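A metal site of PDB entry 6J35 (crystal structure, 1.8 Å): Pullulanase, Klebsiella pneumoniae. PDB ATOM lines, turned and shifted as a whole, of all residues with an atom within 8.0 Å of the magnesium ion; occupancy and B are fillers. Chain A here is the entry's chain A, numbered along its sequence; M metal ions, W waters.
The magnesium ion is bound by the backbone carbonyl oxygen of Asp 973, water W1, the side-chain carboxylate of Asp 964, the side-chain amide oxygen of Gln 1040, the backbone carbonyl oxygen of Val 976 and the side-chain hydroxyl of Ser 971.
Within 4 Å of the magnesium ion: Asp 964, Ser 971, Asp 973, Val 976 and Gln 1040.
The nearest printed residue that does not touch the magnesium ion is Asp 977 (4.1 Å).
The side-chain amide nitrogen (NE2) of Gln 1044 sits at hydrogen-bond distance from the backbone carbonyl oxygen (O) of Asp 964 (2.8 Å).
The backbone carbonyl oxygen (O) of Arg 975 lies within hydrogen-bond range of the backbone NH (N) of Gln 1040, at 2.9 Å.
The backbone NH (N) of Asp 964 sits at hydrogen-bond distance from the backbone carbonyl oxygen (O) of Asp 977.
The side-chain carboxylate of Asp 973 is in hydrogen-bond range of the backbone NH of Arg 975, 3.1 Å away.
The backbone NH (N) of Ser 971 sits close to the side-chain amide nitrogen (NE2) of Gln 1044, 3.3 Å away.
The side-chain amide oxygen (OE1) of Gln 1040 lies close to the backbone carbonyl oxygen (O) of Ser 974.
The side-chain hydroxyl (OG) of Ser 929 is in hydrogen-bond range of the side-chain carboxylate (OD2) of Asp 973 (2.6 Å).
OD1 of Asp 964 lies within hydrogen-bond range of N of Leu 972 (2.9 Å).
Water W1 bridges the side-chain carboxylate (OD1) of Asp 977 (2.7 Å) and the backbone carbonyl oxygen (O) of Asp 964 (2.7 Å).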
ATOM      1  N   SER A 929     -26.915   8.274 -11.568  1.00  0.00           N
ATOM      2  CA  SER A 929     -27.304   8.476 -12.978  1.00  0.00           C
ATOM      3  C   SER A 929     -28.814   8.600 -13.103  1.00  0.00           C
ATOM      4  O   SER A 929     -29.559   7.829 -12.480  1.00  0.00           O
ATOM      5  CB  SER A 929     -26.828   7.328 -13.873  1.00  0.00           C
ATOM      6  OG  SER A 929     -27.276   7.500 -15.215  1.00  0.00           O
ATOM      7  N   PRO A 930     -29.300   9.539 -13.909  1.00  0.00           N
ATOM      8  CA  PRO A 930     -30.738   9.604 -14.196  1.00  0.00           C
ATOM      9  C   PRO A 930     -31.292   8.413 -14.969  1.00  0.00           C
ATOM     10  O   PRO A 930     -32.524   8.289 -15.078  1.00  0.00           O
ATOM     11  CB  PRO A 930     -30.865  10.898 -15.024  1.00  0.00           C
ATOM     12  CG  PRO A 930     -29.544  11.071 -15.668  1.00  0.00           C
ATOM     13  CD  PRO A 930     -28.551  10.614 -14.598  1.00  0.00           C
ATOM     14  N   LEU A 931     -30.443   7.557 -15.548  1.00  0.00           N
ATOM     15  CA  LEU A 931     -30.981   6.405 -16.270  1.00  0.00           C
ATOM     16  C   LEU A 931     -31.656   5.408 -15.320  1.00  0.00           C
ATOM     17  O   LEU A 931     -32.531   4.646 -15.751  1.00  0.00           O
ATOM     18  CB  LEU A 931     -29.868   5.737 -17.094  1.00  0.00           C
ATOM     19  CG  LEU A 931     -29.209   6.650 -18.133  1.00  0.00           C
ATOM     20  CD1 LEU A 931     -27.919   6.042 -18.671  1.00  0.00           C
ATOM     21  CD2 LEU A 931     -30.172   6.950 -19.278  1.00  0.00           C
ATOM     22  N   ARG A 943     -36.244   2.643 -23.446  1.00  0.00           N
ATOM     23  CA  ARG A 943     -34.840   2.531 -23.049  1.00  0.00           C
ATOM     24  C   ARG A 943     -34.485   1.250 -22.303  1.00  0.00           C
ATOM     25  O   ARG A 943     -33.316   0.859 -22.336  1.00  0.00           O
ATOM     26  CB  ARG A 943     -34.430   3.733 -22.181  1.00  0.00           C
ATOM     27  CG  ARG A 943     -34.484   5.085 -22.891  1.00  0.00           C
ATOM     28  CD  ARG A 943     -34.127   6.234 -21.936  1.00  0.00           C
ATOM     29  NE  ARG A 943     -34.158   7.524 -22.626  1.00  0.00           N
ATOM     30  CZ  ARG A 943     -33.098   8.248 -22.962  1.00  0.00           C
ATOM     31  NH1 ARG A 943     -31.881   7.849 -22.646  1.00  0.00           N
ATOM     32  NH2 ARG A 943     -33.247   9.423 -23.576  1.00  0.00           N
ATOM     33  N   ASP A 963     -30.830   2.163 -22.106  1.00  0.00           N
ATOM     34  CA  ASP A 963     -30.229   2.838 -23.248  1.00  0.00           C
ATOM     35  C   ASP A 963     -30.095   4.338 -22.996  1.00  0.00           C
ATOM     36  O   ASP A 963     -31.048   4.983 -22.542  1.00  0.00           O
ATOM     37  CB  ASP A 963     -31.108   2.578 -24.474  1.00  0.00           C
ATOM     38  CG  ASP A 963     -30.439   2.945 -25.780  1.00  0.00           C
ATOM     39  OD1 ASP A 963     -29.215   3.218 -25.801  1.00  0.00           O
ATOM     40  OD2 ASP A 963     -31.179   2.942 -26.793  1.00  0.00           O
ATOM     41  N   ASP A 964     -28.916   4.895 -23.284  1.00  0.00           N
ATOM     42  CA  ASP A 964     -28.786   6.338 -23.432  1.00  0.00           C
ATOM     43  C   ASP A 964     -28.288   6.732 -24.828  1.00  0.00           C
ATOM     44  O   ASP A 964     -27.867   7.883 -25.017  1.00  0.00           O
ATOM     45  CB  ASP A 964     -27.866   6.941 -22.361  1.00  0.00           C
ATOM     46  CG  ASP A 964     -28.208   8.402 -22.044  1.00  0.00           C
ATOM     47  OD1 ASP A 964     -29.404   8.771 -22.113  1.00  0.00           O
ATOM     48  OD2 ASP A 964     -27.277   9.200 -21.745  1.00  0.00           O
ATOM     49  N   GLY A 965     -28.314   5.796 -25.791  1.00  0.00           N
ATOM     50  CA  GLY A 965     -27.794   6.061 -27.121  1.00  0.00           C
ATOM     51  C   GLY A 965     -28.805   6.675 -28.079  1.00  0.00           C
ATOM     52  O   GLY A 965     -29.962   6.946 -27.753  1.00  0.00           O
ATOM     53  N   ALA A 970     -32.525  11.726 -26.544  1.00  0.00           N
ATOM     54  CA  ALA A 970     -31.412  12.543 -26.109  1.00  0.00           C
ATOM     55  C   ALA A 970     -30.595  11.826 -25.049  1.00  0.00           C
ATOM     56  O   ALA A 970     -31.082  10.936 -24.350  1.00  0.00           O
ATOM     57  CB  ALA A 970     -31.919  13.886 -25.563  1.00  0.00           C
ATOM     58  N   SER A 971     -29.340  12.223 -24.929  1.00  0.00           N
ATOM     59  CA  SER A 971     -28.506  11.737 -23.831  1.00  0.00           C
ATOM     60  C   SER A 971     -28.962  12.398 -22.536  1.00  0.00           C
ATOM     61  O   SER A 971     -28.956  13.622 -22.420  1.00  0.00           O
ATOM     62  CB  SER A 971     -27.033  12.059 -24.116  1.00  0.00           C
ATOM     63  OG  SER A 971     -26.199  11.809 -22.995  1.00  0.00           O
ATOM     64  N   LEU A 972     -29.390  11.573 -21.577  1.00  0.00           N
ATOM     65  CA  LEU A 972     -29.779  12.052 -20.258  1.00  0.00           C
ATOM     66  C   LEU A 972     -28.606  12.114 -19.296  1.00  0.00           C
ATOM     67  O   LEU A 972     -28.736  12.741 -18.237  1.00  0.00           O
ATOM     68  CB  LEU A 972     -30.857  11.139 -19.681  1.00  0.00           C
ATOM     69  CG  LEU A 972     -32.109  10.957 -20.523  1.00  0.00           C
ATOM     70  CD1 LEU A 972     -33.020   9.969 -19.808  1.00  0.00           C
ATOM     71  CD2 LEU A 972     -32.796  12.312 -20.684  1.00  0.00           C
ATOM     72  N   ASP A 973     -27.480  11.518 -19.657  1.00  0.00           N
ATOM     73  CA  ASP A 973     -26.331  11.361 -18.775  1.00  0.00           C
ATOM     74  C   ASP A 973     -25.104  11.559 -19.655  1.00  0.00           C
ATOM     75  O   ASP A 973     -24.825  10.716 -20.525  1.00  0.00           O
ATOM     76  CB  ASP A 973     -26.358   9.971 -18.120  1.00  0.00           C
ATOM     77  CG  ASP A 973     -25.234   9.739 -17.114  1.00  0.00           C
ATOM     78  OD1 ASP A 973     -24.245  10.503 -17.076  1.00  0.00           O
ATOM     79  OD2 ASP A 973     -25.361   8.749 -16.355  1.00  0.00           O
ATOM     80  N   SER A 974     -24.389  12.666 -19.474  1.00  0.00           N
ATOM     81  CA  SER A 974     -23.270  12.967 -20.361  1.00  0.00           C
ATOM     82  C   SER A 974     -22.097  12.015 -20.202  1.00  0.00           C
ATOM     83  O   SER A 974     -21.212  11.981 -21.068  1.00  0.00           O
ATOM     84  CB  SER A 974     -22.801  14.420 -20.119  1.00  0.00           C
ATOM     85  OG  SER A 974     -22.266  14.556 -18.819  1.00  0.00           O
ATOM     86  N   ARG A 975     -22.047  11.240 -19.117  1.00  0.00           N
ATOM     87  CA  ARG A 975     -20.907  10.369 -18.871  1.00  0.00           C
ATOM     88  C   ARG A 975     -21.017   9.018 -19.541  1.00  0.00           C
ATOM     89  O   ARG A 975     -19.988   8.388 -19.772  1.00  0.00           O
ATOM     90  CB  ARG A 975     -20.714  10.162 -17.363  1.00  0.00           C
ATOM     91  CG  ARG A 975     -20.448  11.457 -16.618  1.00  0.00           C
ATOM     92  CD  ARG A 975     -19.835  11.237 -15.257  1.00  0.00           C
ATOM     93  NE  ARG A 975     -19.693  12.495 -14.525  1.00  0.00           N
ATOM     94  CZ  ARG A 975     -19.159  12.593 -13.311  1.00  0.00           C
ATOM     95  NH1 ARG A 975     -19.052  13.778 -12.718  1.00  0.00           N
ATOM     96  NH2 ARG A 975     -18.716  11.484 -12.690  1.00  0.00           N
ATOM     97  N   VAL A 976     -22.222   8.544 -19.867  1.00  0.00           N
ATOM     98  CA  VAL A 976     -22.400   7.183 -20.363  1.00  0.00           C
ATOM     99  C   VAL A 976     -23.413   7.178 -21.500  1.00  0.00           C
ATOM    100  O   VAL A 976     -24.289   8.044 -21.594  1.00  0.00           O
ATOM    101  CB  VAL A 976     -22.858   6.178 -19.277  1.00  0.00           C
ATOM    102  CG1 VAL A 976     -21.950   6.225 -18.044  1.00  0.00           C
ATOM    103  CG2 VAL A 976     -24.314   6.398 -18.887  1.00  0.00           C
ATOM    104  N   ASP A 977     -23.296   6.149 -22.340  1.00  0.00           N
ATOM    105  CA  ASP A 977     -24.223   5.859 -23.435  1.00  0.00           C
ATOM    106  C   ASP A 977     -25.179   4.736 -23.089  1.00  0.00           C
ATOM    107  O   ASP A 977     -26.036   4.383 -23.907  1.00  0.00           O
ATOM    108  CB  ASP A 977     -23.446   5.485 -24.700  1.00  0.00           C
ATOM    109  CG  ASP A 977     -22.856   6.695 -25.412  1.00  0.00           C
ATOM    110  OD1 ASP A 977     -23.494   7.770 -25.433  1.00  0.00           O
ATOM    111  OD2 ASP A 977     -21.744   6.561 -25.968  1.00  0.00           O
ATOM    112  N   GLY A 978     -25.056   4.165 -21.908  1.00  0.00           N
ATOM    113  CA  GLY A 978     -25.905   3.065 -21.521  1.00  0.00           C
ATOM    114  C   GLY A 978     -25.399   2.413 -20.251  1.00  0.00           C
ATOM    115  O   GLY A 978     -24.240   2.604 -19.873  1.00  0.00           O
ATOM    116  N   LEU A1038     -21.346   2.059 -20.687  1.00  0.00           N
ATOM    117  CA  LEU A1038     -20.679   2.406 -21.923  1.00  0.00           C
ATOM    118  C   LEU A1038     -20.200   3.841 -21.802  1.00  0.00           C
ATOM    119  O   LEU A1038     -21.035   4.756 -21.752  1.00  0.00           O
ATOM    120  CB  LEU A1038     -21.640   2.261 -23.106  1.00  0.00           C
ATOM    121  CG  LEU A1038     -22.150   0.849 -23.418  1.00  0.00           C
ATOM    122  CD1 LEU A1038     -23.185   0.899 -24.526  1.00  0.00           C
ATOM    123  CD2 LEU A1038     -20.988  -0.092 -23.797  1.00  0.00           C
ATOM    124  N   PRO A1039     -18.897   4.104 -21.735  1.00  0.00           N
ATOM    125  CA  PRO A1039     -18.432   5.490 -21.574  1.00  0.00           C
ATOM    126  C   PRO A1039     -18.818   6.339 -22.783  1.00  0.00           C
ATOM    127  O   PRO A1039     -18.706   5.900 -23.921  1.00  0.00           O
ATOM    128  CB  PRO A1039     -16.904   5.345 -21.478  1.00  0.00           C
ATOM    129  CG  PRO A1039     -16.615   4.081 -22.228  1.00  0.00           C
ATOM    130  CD  PRO A1039     -17.776   3.166 -21.931  1.00  0.00           C
ATOM    131  N   GLN A1040     -19.270   7.574 -22.514  1.00  0.00           N
ATOM    132  CA  GLN A1040     -19.707   8.445 -23.604  1.00  0.00           C
ATOM    133  C   GLN A1040     -18.533   9.281 -24.101  1.00  0.00           C
ATOM    134  O   GLN A1040     -17.771   9.831 -23.294  1.00  0.00           O
ATOM    135  CB  GLN A1040     -20.841   9.362 -23.161  1.00  0.00           C
ATOM    136  CG  GLN A1040     -21.489  10.163 -24.297  1.00  0.00           C
ATOM    137  CD  GLN A1040     -22.746  10.880 -23.845  1.00  0.00           C
ATOM    138  OE1 GLN A1040     -23.421  10.410 -22.918  1.00  0.00           O
ATOM    139  NE2 GLN A1040     -23.064  12.010 -24.467  1.00  0.00           N
ATOM    140  N   GLY A1041     -18.381   9.348 -25.417  1.00  0.00           N
ATOM    141  CA  GLY A1041     -17.275  10.056 -26.035  1.00  0.00           C
ATOM    142  C   GLY A1041     -17.679  11.424 -26.538  1.00  0.00           C
ATOM    143  O   GLY A1041     -18.510  12.113 -25.936  1.00  0.00           O
ATOM    144  N   SER A1043     -19.455  12.465 -29.097  1.00  0.00           N
ATOM    145  CA  SER A1043     -20.883  12.574 -29.311  1.00  0.00           C
ATOM    146  C   SER A1043     -21.594  11.394 -28.674  1.00  0.00           C
ATOM    147  O   SER A1043     -20.989  10.353 -28.392  1.00  0.00           O
ATOM    148  CB  SER A1043     -21.228  12.603 -30.818  1.00  0.00           C
ATOM    149  OG  SER A1043     -20.392  13.493 -31.524  1.00  0.00           O
ATOM    150  N   GLN A1044     -22.901  11.544 -28.486  1.00  0.00           N
ATOM    151  CA  GLN A1044     -23.732  10.423 -28.113  1.00  0.00           C
ATOM    152  C   GLN A1044     -23.478   9.232 -29.039  1.00  0.00           C
ATOM    153  O   GLN A1044     -23.368   9.391 -30.268  1.00  0.00           O
ATOM    154  CB  GLN A1044     -25.203  10.842 -28.148  1.00  0.00           C
ATOM    155  CG  GLN A1044     -26.190   9.740 -27.809  1.00  0.00           C
ATOM    156  CD  GLN A1044     -27.631  10.192 -27.919  1.00  0.00           C
ATOM    157  OE1 GLN A1044     -28.004  10.906 -28.849  1.00  0.00           O
ATOM    158  NE2 GLN A1044     -28.453   9.758 -26.975  1.00  0.00           N
ATOM    159  N   GLY A1045     -23.375   8.038 -28.456  1.00  0.00           N
ATOM    160  CA  GLY A1045     -23.046   6.834 -29.181  1.00  0.00           C
ATOM    161  C   GLY A1045     -24.225   5.907 -29.410  1.00  0.00           C
ATOM    162  O   GLY A1045     -25.390   6.264 -29.237  1.00  0.00           O
HETATM  163 MG    MG M   1     -25.342   9.788 -22.314  1.00  0.00          MG
HETATM  164  O   HOH W   1     -25.537   9.048 -24.268  1.00  0.00           O
